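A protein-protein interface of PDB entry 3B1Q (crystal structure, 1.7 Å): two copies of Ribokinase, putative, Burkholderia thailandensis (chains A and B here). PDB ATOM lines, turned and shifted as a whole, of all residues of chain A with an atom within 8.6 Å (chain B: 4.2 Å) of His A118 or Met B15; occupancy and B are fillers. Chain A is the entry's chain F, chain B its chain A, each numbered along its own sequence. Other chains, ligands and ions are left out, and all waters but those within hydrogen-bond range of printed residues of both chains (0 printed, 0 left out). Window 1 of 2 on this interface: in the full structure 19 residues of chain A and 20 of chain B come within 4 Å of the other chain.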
ATOM      1  N   SER A   8      13.375   4.220 -19.446  1.00  0.00           N
ATOM      2  CA  SER A   8      13.111   3.610 -20.718  1.00  0.00           C
ATOM      3  C   SER A   8      13.288   4.582 -21.863  1.00  0.00           C
ATOM      4  O   SER A   8      13.082   5.827 -21.720  1.00  0.00           O
ATOM      5  CB  SER A   8      11.699   2.975 -20.732  1.00  0.00           C
ATOM      6  OG  SER A   8      10.707   3.974 -20.438  1.00  0.00           O
ATOM      7  N   ILE A   9      13.659   4.018 -23.025  1.00  0.00           N
ATOM      8  CA  ILE A   9      13.664   4.800 -24.257  1.00  0.00           C
ATOM      9  C   ILE A   9      12.868   3.988 -25.226  1.00  0.00           C
ATOM     10  O   ILE A   9      13.187   2.834 -25.440  1.00  0.00           O
ATOM     11  CB  ILE A   9      15.090   5.029 -24.813  1.00  0.00           C
ATOM     12  CG1 ILE A   9      16.045   5.579 -23.722  1.00  0.00           C
ATOM     13  CG2 ILE A   9      15.057   5.973 -25.941  1.00  0.00           C
ATOM     14  CD1 ILE A   9      17.558   5.518 -24.160  1.00  0.00           C
ATOM     15  N   ALA A  10      11.774   4.562 -25.752  1.00  0.00           N
ATOM     16  CA  ALA A  10      10.765   3.671 -26.409  1.00  0.00           C
ATOM     17  C   ALA A  10      10.032   4.372 -27.511  1.00  0.00           C
ATOM     18  O   ALA A  10       9.995   5.581 -27.509  1.00  0.00           O
ATOM     19  CB  ALA A  10       9.743   3.158 -25.303  1.00  0.00           C
ATOM     20  N   TYR A  11       9.453   3.631 -28.463  1.00  0.00           N
ATOM     21  CA  TYR A  11       8.506   4.221 -29.383  1.00  0.00           C
ATOM     22  C   TYR A  11       7.118   3.946 -28.845  1.00  0.00           C
ATOM     23  O   TYR A  11       6.829   2.814 -28.443  1.00  0.00           O
ATOM     24  CB  TYR A  11       8.659   3.609 -30.765  1.00  0.00           C
ATOM     25  CG  TYR A  11      10.046   3.849 -31.328  1.00  0.00           C
ATOM     26  CD1 TYR A  11      10.433   5.138 -31.706  1.00  0.00           C
ATOM     27  CD2 TYR A  11      10.955   2.786 -31.512  1.00  0.00           C
ATOM     28  CE1 TYR A  11      11.720   5.400 -32.209  1.00  0.00           C
ATOM     29  CE2 TYR A  11      12.271   3.041 -32.030  1.00  0.00           C
ATOM     30  CZ  TYR A  11      12.615   4.341 -32.390  1.00  0.00           C
ATOM     31  OH  TYR A  11      13.869   4.636 -32.916  1.00  0.00           O
ATOM     32  N   ASN A  13       3.056   3.856 -29.534  1.00  0.00           N
ATOM     33  CA  ASN A  13       2.085   3.648 -30.590  1.00  0.00           C
ATOM     34  C   ASN A  13       0.749   3.920 -29.940  1.00  0.00           C
ATOM     35  O   ASN A  13       0.276   3.138 -29.097  1.00  0.00           O
ATOM     36  CB  ASN A  13       2.178   2.237 -31.092  1.00  0.00           C
ATOM     37  CG  ASN A  13       3.550   1.949 -31.655  1.00  0.00           C
ATOM     38  OD1 ASN A  13       3.854   2.360 -32.777  1.00  0.00           O
ATOM     39  ND2 ASN A  13       4.439   1.331 -30.830  1.00  0.00           N
ATOM     40  N   MET A  15      -2.875   4.192 -30.092  1.00  0.00           N
ATOM     41  CA  MET A  15      -3.976   3.615 -30.861  1.00  0.00           C
ATOM     42  C   MET A  15      -5.307   4.123 -30.318  1.00  0.00           C
ATOM     43  O   MET A  15      -5.519   4.126 -29.100  1.00  0.00           O
ATOM     44  CB  MET A  15      -3.966   2.069 -30.807  1.00  0.00           C
ATOM     45  CG  MET A  15      -2.597   1.423 -30.996  1.00  0.00           C
ATOM     46  SD  MET A  15      -2.737  -0.326 -31.517  1.00  0.00           S
ATOM     47  CE  MET A  15      -2.754  -1.219 -29.946  1.00  0.00           C
ATOM     48  N   TYR A  99      15.347  -5.400 -30.603  1.00  0.00           N
ATOM     49  CA  TYR A  99      14.364  -4.342 -30.869  1.00  0.00           C
ATOM     50  C   TYR A  99      14.303  -3.341 -29.734  1.00  0.00           C
ATOM     51  O   TYR A  99      14.437  -3.727 -28.546  1.00  0.00           O
ATOM     52  CB  TYR A  99      12.986  -4.996 -30.985  1.00  0.00           C
ATOM     53  CG  TYR A  99      12.843  -5.802 -32.245  1.00  0.00           C
ATOM     54  CD1 TYR A  99      12.401  -5.195 -33.402  1.00  0.00           C
ATOM     55  CD2 TYR A  99      13.107  -7.171 -32.264  1.00  0.00           C
ATOM     56  CE1 TYR A  99      12.277  -5.911 -34.628  1.00  0.00           C
ATOM     57  CE2 TYR A  99      13.002  -7.913 -33.482  1.00  0.00           C
ATOM     58  CZ  TYR A  99      12.582  -7.268 -34.641  1.00  0.00           C
ATOM     59  OH  TYR A  99      12.400  -7.940 -35.805  1.00  0.00           O
ATOM     60  N   SER A 100      14.043  -2.083 -30.089  1.00  0.00           N
ATOM     61  CA  SER A 100      13.754  -1.035 -29.071  1.00  0.00           C
ATOM     62  C   SER A 100      12.440  -1.312 -28.359  1.00  0.00           C
ATOM     63  O   SER A 100      11.543  -1.949 -28.904  1.00  0.00           O
ATOM     64  CB  SER A 100      13.758   0.346 -29.702  1.00  0.00           C
ATOM     65  OG  SER A 100      15.021   0.575 -30.293  1.00  0.00           O
ATOM     66  N   ALA A 101      12.348  -0.876 -27.107  1.00  0.00           N
ATOM     67  CA  ALA A 101      11.074  -0.954 -26.384  1.00  0.00           C
ATOM     68  C   ALA A 101       9.946  -0.290 -27.187  1.00  0.00           C
ATOM     69  O   ALA A 101      10.158   0.722 -27.823  1.00  0.00           O
ATOM     70  CB  ALA A 101      11.221  -0.230 -25.027  1.00  0.00           C
ATOM     71  N   GLN A 102       8.753  -0.885 -27.154  1.00  0.00           N
ATOM     72  CA  GLN A 102       7.593  -0.180 -27.707  1.00  0.00           C
ATOM     73  C   GLN A 102       6.418  -0.295 -26.752  1.00  0.00           C
ATOM     74  O   GLN A 102       6.189  -1.340 -26.156  1.00  0.00           O
ATOM     75  CB  GLN A 102       7.184  -0.750 -29.060  1.00  0.00           C
ATOM     76  CG  GLN A 102       8.277  -0.521 -30.200  1.00  0.00           C
ATOM     77  CD  GLN A 102       7.722  -0.276 -31.544  1.00  0.00           C
ATOM     78  OE1 GLN A 102       6.752   0.445 -31.707  1.00  0.00           O
ATOM     79  NE2 GLN A 102       8.358  -0.849 -32.548  1.00  0.00           N
ATOM     80  N   ALA A 103       5.676   0.797 -26.652  1.00  0.00           N
ATOM     81  CA  ALA A 103       4.455   0.849 -25.843  1.00  0.00           C
ATOM     82  C   ALA A 103       3.280   0.823 -26.826  1.00  0.00           C
ATOM     83  O   ALA A 103       3.222   1.659 -27.742  1.00  0.00           O
ATOM     84  CB  ALA A 103       4.445   2.154 -24.995  1.00  0.00           C
ATOM     85  N   MET A 104       2.391  -0.162 -26.682  1.00  0.00           N
ATOM     86  CA  MET A 104       1.155  -0.206 -27.461  1.00  0.00           C
ATOM     87  C   MET A 104       0.095   0.408 -26.578  1.00  0.00           C
ATOM     88  O   MET A 104      -0.398  -0.240 -25.652  1.00  0.00           O
ATOM     89  CB  MET A 104       0.802  -1.645 -27.845  1.00  0.00           C
ATOM     90  CG  MET A 104       1.806  -2.291 -28.697  1.00  0.00           C
ATOM     91  SD  MET A 104       2.058  -1.192 -30.096  1.00  0.00           S
ATOM     92  CE  MET A 104       0.596  -1.430 -31.115  1.00  0.00           C
ATOM     93  N   ILE A 105      -0.230   1.665 -26.839  1.00  0.00           N
ATOM     94  CA  ILE A 105      -1.065   2.449 -25.944  1.00  0.00           C
ATOM     95  C   ILE A 105      -2.464   2.554 -26.602  1.00  0.00           C
ATOM     96  O   ILE A 105      -2.643   3.307 -27.579  1.00  0.00           O
ATOM     97  CB  ILE A 105      -0.414   3.816 -25.664  1.00  0.00           C
ATOM     98  CG1 ILE A 105       1.055   3.671 -25.148  1.00  0.00           C
ATOM     99  CG2 ILE A 105      -1.266   4.627 -24.664  1.00  0.00           C
ATOM    100  CD1 ILE A 105       1.783   4.936 -24.813  1.00  0.00           C
ATOM    101  N   THR A 115      -1.963   0.188 -21.686  1.00  0.00           N
ATOM    102  CA  THR A 115      -0.677  -0.060 -22.389  1.00  0.00           C
ATOM    103  C   THR A 115      -0.222  -1.539 -22.313  1.00  0.00           C
ATOM    104  O   THR A 115      -0.161  -2.112 -21.227  1.00  0.00           O
ATOM    105  CB  THR A 115       0.420   0.875 -21.845  1.00  0.00           C
ATOM    106  OG1 THR A 115       0.019   2.238 -22.043  1.00  0.00           O
ATOM    107  CG2 THR A 115       1.825   0.660 -22.497  1.00  0.00           C
ATOM    108  N   ALA A 116       0.086  -2.141 -23.462  1.00  0.00           N
ATOM    109  CA  ALA A 116       0.914  -3.355 -23.492  1.00  0.00           C
ATOM    110  C   ALA A 116       2.325  -2.845 -23.781  1.00  0.00           C
ATOM    111  O   ALA A 116       2.548  -2.237 -24.835  1.00  0.00           O
ATOM    112  CB  ALA A 116       0.443  -4.337 -24.599  1.00  0.00           C
ATOM    113  N   PHE A 117       3.270  -3.052 -22.859  1.00  0.00           N
ATOM    114  CA  PHE A 117       4.612  -2.549 -23.065  1.00  0.00           C
ATOM    115  C   PHE A 117       5.539  -3.705 -23.409  1.00  0.00           C
ATOM    116  O   PHE A 117       5.660  -4.669 -22.651  1.00  0.00           O
ATOM    117  CB  PHE A 117       5.128  -1.857 -21.800  1.00  0.00           C
ATOM    118  CG  PHE A 117       6.412  -1.094 -22.013  1.00  0.00           C
ATOM    119  CD1 PHE A 117       6.383   0.173 -22.591  1.00  0.00           C
ATOM    120  CD2 PHE A 117       7.646  -1.619 -21.607  1.00  0.00           C
ATOM    121  CE1 PHE A 117       7.531   0.896 -22.829  1.00  0.00           C
ATOM    122  CE2 PHE A 117       8.825  -0.876 -21.815  1.00  0.00           C
ATOM    123  CZ  PHE A 117       8.770   0.379 -22.423  1.00  0.00           C
ATOM    124  N   HIS A 118       6.229  -3.596 -24.549  1.00  0.00           N
ATOM    125  CA  HIS A 118       7.050  -4.698 -25.019  1.00  0.00           C
ATOM    126  C   HIS A 118       8.461  -4.217 -24.777  1.00  0.00           C
ATOM    127  O   HIS A 118       8.918  -3.365 -25.540  1.00  0.00           O
ATOM    128  CB  HIS A 118       6.866  -4.859 -26.531  1.00  0.00           C
ATOM    129  CG  HIS A 118       5.464  -5.169 -26.946  1.00  0.00           C
ATOM    130  ND1 HIS A 118       4.415  -4.272 -26.793  1.00  0.00           N
ATOM    131  CD2 HIS A 118       4.926  -6.285 -27.486  1.00  0.00           C
ATOM    132  CE1 HIS A 118       3.295  -4.830 -27.227  1.00  0.00           C
ATOM    133  NE2 HIS A 118       3.584  -6.043 -27.668  1.00  0.00           N
ATOM    134  N   PRO A 119       9.146  -4.724 -23.742  1.00  0.00           N
ATOM    135  CA  PRO A 119      10.380  -4.018 -23.319  1.00  0.00           C
ATOM    136  C   PRO A 119      11.578  -4.114 -24.273  1.00  0.00           C
ATOM    137  O   PRO A 119      12.394  -3.190 -24.267  1.00  0.00           O
ATOM    138  CB  PRO A 119      10.710  -4.680 -21.960  1.00  0.00           C
ATOM    139  CG  PRO A 119      10.038  -6.014 -22.000  1.00  0.00           C
ATOM    140  CD  PRO A 119       8.781  -5.800 -22.806  1.00  0.00           C
ATOM    141  N   GLY A 120      11.734  -5.231 -24.989  1.00  0.00           N
ATOM    142  CA  GLY A 120      12.835  -5.365 -25.965  1.00  0.00           C
ATOM    143  C   GLY A 120      14.138  -5.035 -25.236  1.00  0.00           C
ATOM    144  O   GLY A 120      14.412  -5.607 -24.173  1.00  0.00           O
ATOM    145  N   ALA A 121      14.910  -4.111 -25.791  1.00  0.00           N
ATOM    146  CA  ALA A 121      16.238  -3.799 -25.243  1.00  0.00           C
ATOM    147  C   ALA A 121      16.219  -3.258 -23.835  1.00  0.00           C
ATOM    148  O   ALA A 121      17.226  -3.337 -23.161  1.00  0.00           O
ATOM    149  CB  ALA A 121      16.985  -2.813 -26.161  1.00  0.00           C
ATOM    150  N   MET A 122      15.095  -2.671 -23.393  1.00  0.00           N
ATOM    151  CA  MET A 122      14.970  -2.211 -21.989  1.00  0.00           C
ATOM    152  C   MET A 122      15.287  -3.323 -20.981  1.00  0.00           C
ATOM    153  O   MET A 122      15.775  -3.056 -19.886  1.00  0.00           O
ATOM    154  CB  MET A 122      13.585  -1.642 -21.707  1.00  0.00           C
ATOM    155  CG  MET A 122      13.504  -0.903 -20.388  1.00  0.00           C
ATOM    156  SD  MET A 122      11.784  -0.557 -19.920  1.00  0.00           S
ATOM    157  CE  MET A 122      11.219  -2.100 -19.173  1.00  0.00           C
ATOM    158  N   MET A 123      15.078  -4.576 -21.371  1.00  0.00           N
ATOM    159  CA  MET A 123      15.358  -5.691 -20.464  1.00  0.00           C
ATOM    160  C   MET A 123      16.856  -5.839 -20.150  1.00  0.00           C
ATOM    161  O   MET A 123      17.231  -6.555 -19.216  1.00  0.00           O
ATOM    162  CB  MET A 123      14.855  -7.028 -21.059  1.00  0.00           C
ATOM    163  CG  MET A 123      13.369  -7.174 -21.111  1.00  0.00           C
ATOM    164  SD  MET A 123      12.512  -6.601 -19.613  1.00  0.00           S
ATOM    165  CE  MET A 123      12.546  -8.070 -18.553  1.00  0.00           C
ATOM    166  N   ASN B  13      -0.059 -10.312 -34.202  1.00  0.00           N
ATOM    167  CA  ASN B  13       1.031 -10.144 -33.266  1.00  0.00           C
ATOM    168  C   ASN B  13       0.470 -10.670 -31.960  1.00  0.00           C
ATOM    169  O   ASN B  13      -0.362  -9.998 -31.331  1.00  0.00           O
ATOM    170  CB  ASN B  13       1.347  -8.678 -33.165  1.00  0.00           C
ATOM    171  CG  ASN B  13       1.695  -8.089 -34.524  1.00  0.00           C
ATOM    172  OD1 ASN B  13       2.843  -8.160 -34.958  1.00  0.00           O
ATOM    173  ND2 ASN B  13       0.692  -7.483 -35.205  1.00  0.00           N
ATOM    174  N   ILE B  14       0.936 -11.859 -31.563  1.00  0.00           N
ATOM    175  CA  ILE B  14       0.266 -12.647 -30.526  1.00  0.00           C
ATOM    176  C   ILE B  14       1.110 -12.672 -29.271  1.00  0.00           C
ATOM    177  O   ILE B  14       2.332 -12.932 -29.291  1.00  0.00           O
ATOM    178  CB  ILE B  14       0.022 -14.091 -31.058  1.00  0.00           C
ATOM    179  CG1 ILE B  14      -0.807 -14.042 -32.332  1.00  0.00           C
ATOM    180  CG2 ILE B  14      -0.730 -14.935 -29.983  1.00  0.00           C
ATOM    181  CD1 ILE B  14      -0.771 -15.369 -33.086  1.00  0.00           C
ATOM    182  N   MET B  15       0.455 -12.293 -28.155  1.00  0.00           N
ATOM    183  CA  MET B  15       1.119 -12.071 -26.865  1.00  0.00           C
ATOM    184  C   MET B  15       0.327 -12.827 -25.808  1.00  0.00           C
ATOM    185  O   MET B  15      -0.877 -13.044 -25.980  1.00  0.00           O
ATOM    186  CB  MET B  15       1.140 -10.569 -26.517  1.00  0.00           C
ATOM    187  CG  MET B  15       1.735  -9.667 -27.614  1.00  0.00           C
ATOM    188  SD  MET B  15       1.322  -7.916 -27.410  1.00  0.00           S
ATOM    189  CE  MET B  15      -0.184  -7.816 -28.365  1.00  0.00           C
ATOM    190  N   THR B  16       1.004 -13.319 -24.773  1.00  0.00           N
ATOM    191  CA  THR B  16       0.281 -13.968 -23.681  1.00  0.00           C
ATOM    192  C   THR B  16       0.228 -13.008 -22.499  1.00  0.00           C
ATOM    193  O   THR B  16       1.131 -12.203 -22.280  1.00  0.00           O
ATOM    194  CB  THR B  16       0.894 -15.328 -23.254  1.00  0.00           C
ATOM    195  OG1 THR B  16       2.284 -15.152 -22.950  1.00  0.00           O
ATOM    196  CG2 THR B  16       0.696 -16.405 -24.350  1.00  0.00           C
ATOM    197  N   VAL B  39       4.614  -7.094 -21.613  1.00  0.00           N
ATOM    198  CA  VAL B  39       4.384  -8.224 -22.495  1.00  0.00           C
ATOM    199  C   VAL B  39       5.772  -8.642 -22.979  1.00  0.00           C
ATOM    200  O   VAL B  39       6.325  -8.034 -23.902  1.00  0.00           O
ATOM    201  CB  VAL B  39       3.491  -7.843 -23.723  1.00  0.00           C
ATOM    202  CG1 VAL B  39       3.696  -8.834 -24.802  1.00  0.00           C
ATOM    203  CG2 VAL B  39       2.007  -7.839 -23.345  1.00  0.00           C
ATOM    204  N   THR B  41       7.027 -11.473 -24.402  1.00  0.00           N
ATOM    205  CA  THR B  41       7.140 -12.192 -25.683  1.00  0.00           C
ATOM    206  C   THR B  41       5.971 -11.868 -26.614  1.00  0.00           C
ATOM    207  O   THR B  41       4.807 -11.836 -26.202  1.00  0.00           O
ATOM    208  CB  THR B  41       7.259 -13.747 -25.504  1.00  0.00           C
ATOM    209  OG1 THR B  41       8.356 -14.026 -24.632  1.00  0.00           O
ATOM    210  CG2 THR B  41       7.587 -14.449 -26.828  1.00  0.00           C
ATOM    211  N   MET B  42       6.304 -11.623 -27.875  1.00  0.00           N
ATOM    212  CA  MET B  42       5.289 -11.451 -28.873  1.00  0.00           C
ATOM    213  C   MET B  42       5.774 -12.327 -30.065  1.00  0.00           C
ATOM    214  O   MET B  42       7.008 -12.428 -30.301  1.00  0.00           O
ATOM    215  CB  MET B  42       5.263  -9.979 -29.259  1.00  0.00           C
ATOM    216  CG  MET B  42       4.275  -9.668 -30.411  1.00  0.00           C
ATOM    217  SD  MET B  42       4.278  -7.898 -30.746  1.00  0.00           S
ATOM    218  CE  MET B  42       5.478  -7.690 -32.089  1.00  0.00           C
ATOM    219  N   MET B 104      -3.367  -7.108 -32.792  1.00  0.00           N
ATOM    220  CA  MET B 104      -2.551  -7.154 -31.592  1.00  0.00           C
ATOM    221  C   MET B 104      -3.336  -8.015 -30.589  1.00  0.00           C
ATOM    222  O   MET B 104      -4.328  -7.554 -29.999  1.00  0.00           O
ATOM    223  CB  MET B 104      -2.292  -5.746 -31.082  1.00  0.00           C
ATOM    224  CG  MET B 104      -0.966  -5.134 -31.519  1.00  0.00           C
ATOM    225  SD  MET B 104      -0.741  -4.919 -33.288  1.00  0.00           S
ATOM    226  CE  MET B 104       1.037  -4.488 -33.319  1.00  0.00           C
ATOM    227  N   ILE B 105      -2.924  -9.267 -30.432  1.00  0.00           N
ATOM    228  CA  ILE B 105      -3.789 -10.320 -29.847  1.00  0.00           C
ATOM    229  C   ILE B 105      -3.151 -10.807 -28.554  1.00  0.00           C
ATOM    230  O   ILE B 105      -1.993 -11.193 -28.546  1.00  0.00           O
ATOM    231  CB  ILE B 105      -3.929 -11.547 -30.793  1.00  0.00           C
ATOM    232  CG1 ILE B 105      -4.541 -11.177 -32.163  1.00  0.00           C
ATOM    233  CG2 ILE B 105      -4.764 -12.680 -30.122  1.00  0.00           C
ATOM    234  CD1 ILE B 105      -4.578 -12.411 -33.182  1.00  0.00           C
ATOM    235  N   THR B 106      -3.876 -10.725 -27.421  1.00  0.00           N
ATOM    236  CA  THR B 106      -3.329 -11.109 -26.126  1.00  0.00           C
ATOM    237  C   THR B 106      -4.184 -12.246 -25.550  1.00  0.00           C
ATOM    238  O   THR B 106      -5.424 -12.169 -25.578  1.00  0.00           O
ATOM    239  CB  THR B 106      -3.367  -9.915 -25.173  1.00  0.00           C
ATOM    240  OG1 THR B 106      -2.493  -8.918 -25.685  1.00  0.00           O
ATOM    241  CG2 THR B 106      -2.865 -10.325 -23.767  1.00  0.00           C
ATOM    242  N   THR B 107      -3.528 -13.299 -25.046  1.00  0.00           N
ATOM    243  CA  THR B 107      -4.237 -14.516 -24.606  1.00  0.00           C
ATOM    244  C   THR B 107      -3.964 -14.656 -23.115  1.00  0.00           C
ATOM    245  O   THR B 107      -2.821 -14.566 -22.677  1.00  0.00           O
ATOM    246  CB  THR B 107      -3.735 -15.806 -25.341  1.00  0.00           C
ATOM    247  OG1 THR B 107      -3.810 -15.611 -26.759  1.00  0.00           O
ATOM    248  CG2 THR B 107      -4.551 -17.050 -24.971  1.00  0.00           C
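A ring nitrogen (NE2) of His A118 is in hydrogen-bond range of the side-chain sulfur of Met B15 (2.9 Å).
N of Val B39 lies within hydrogen-bond range of O of Phe A117, 2.8 Å away.
A ring nitrogen (NE2) of His A118 sits at hydrogen-bond distance from the side-chain sulfur of Met B42 (3.7 Å).
ND2 of Asn B13 lies within hydrogen-bond range of SD of Met B104 (3.5 Å).
The backbone carbonyl oxygen (O) of Ile B105 lies within hydrogen-bond range of the backbone NH (N) of Met B15 (2.7 Å).
ND2 of Asn A13 sits at hydrogen-bond distance from SD of Met A104 (3.5 Å).
The backbone NH (N) of His A118 lies within hydrogen-bond range of the backbone carbonyl oxygen (O) of Gln A102 (2.8 Å).
The backbone NH of Met A104 is in hydrogen-bond range of the backbone carbonyl oxygen of Ala A116 (2.8 Å).
A ring nitrogen (ND1) of His A118 lies within hydrogen-bond range of the backbone carbonyl oxygen of Ala A116 (3.4 Å).
Printed residues of chain B that touch a printed residue of chain A: Met B15, Val B39, Met B42 and Met B104.
Met A104 touches Met B104.
His A118 touches Val B39 (CA to O, 3.6 Å).
Val B39 touches Pro A119 (O to CD, 3.5 Å).
Met A104 touches its own counterpart, Met B104.
Of the 6 pairs that touch across the chains among the printed residues, 1 has its exchanged pair printed and touching as well.
His A118 touches three residues of chain B.
Of chain A, only His A118 comes within 4 Å of Met B15.
No residue of chain A comes within 4 Å of Thr B16.
Of the printed residues of chain A, Val B39 touches Phe A117, His A118 and Pro A119.
Printed residues of chain B within 4 Å of Phe A117: Val B39 (2.8 Å).
Printed residues of chain A within 4 Å of Met B104: Met A104 (3.8 Å).
Gly A120 touches none of the printed residues of chain B.
Ala A10 touches none of the printed residues of chain B.
The nearest residue of chain A that does not touch Met B15 is Ala A116 (4.6 Å).
The nearest printed residue of chain B that does not touch Met A104 is Met B15 (5.8 Å).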
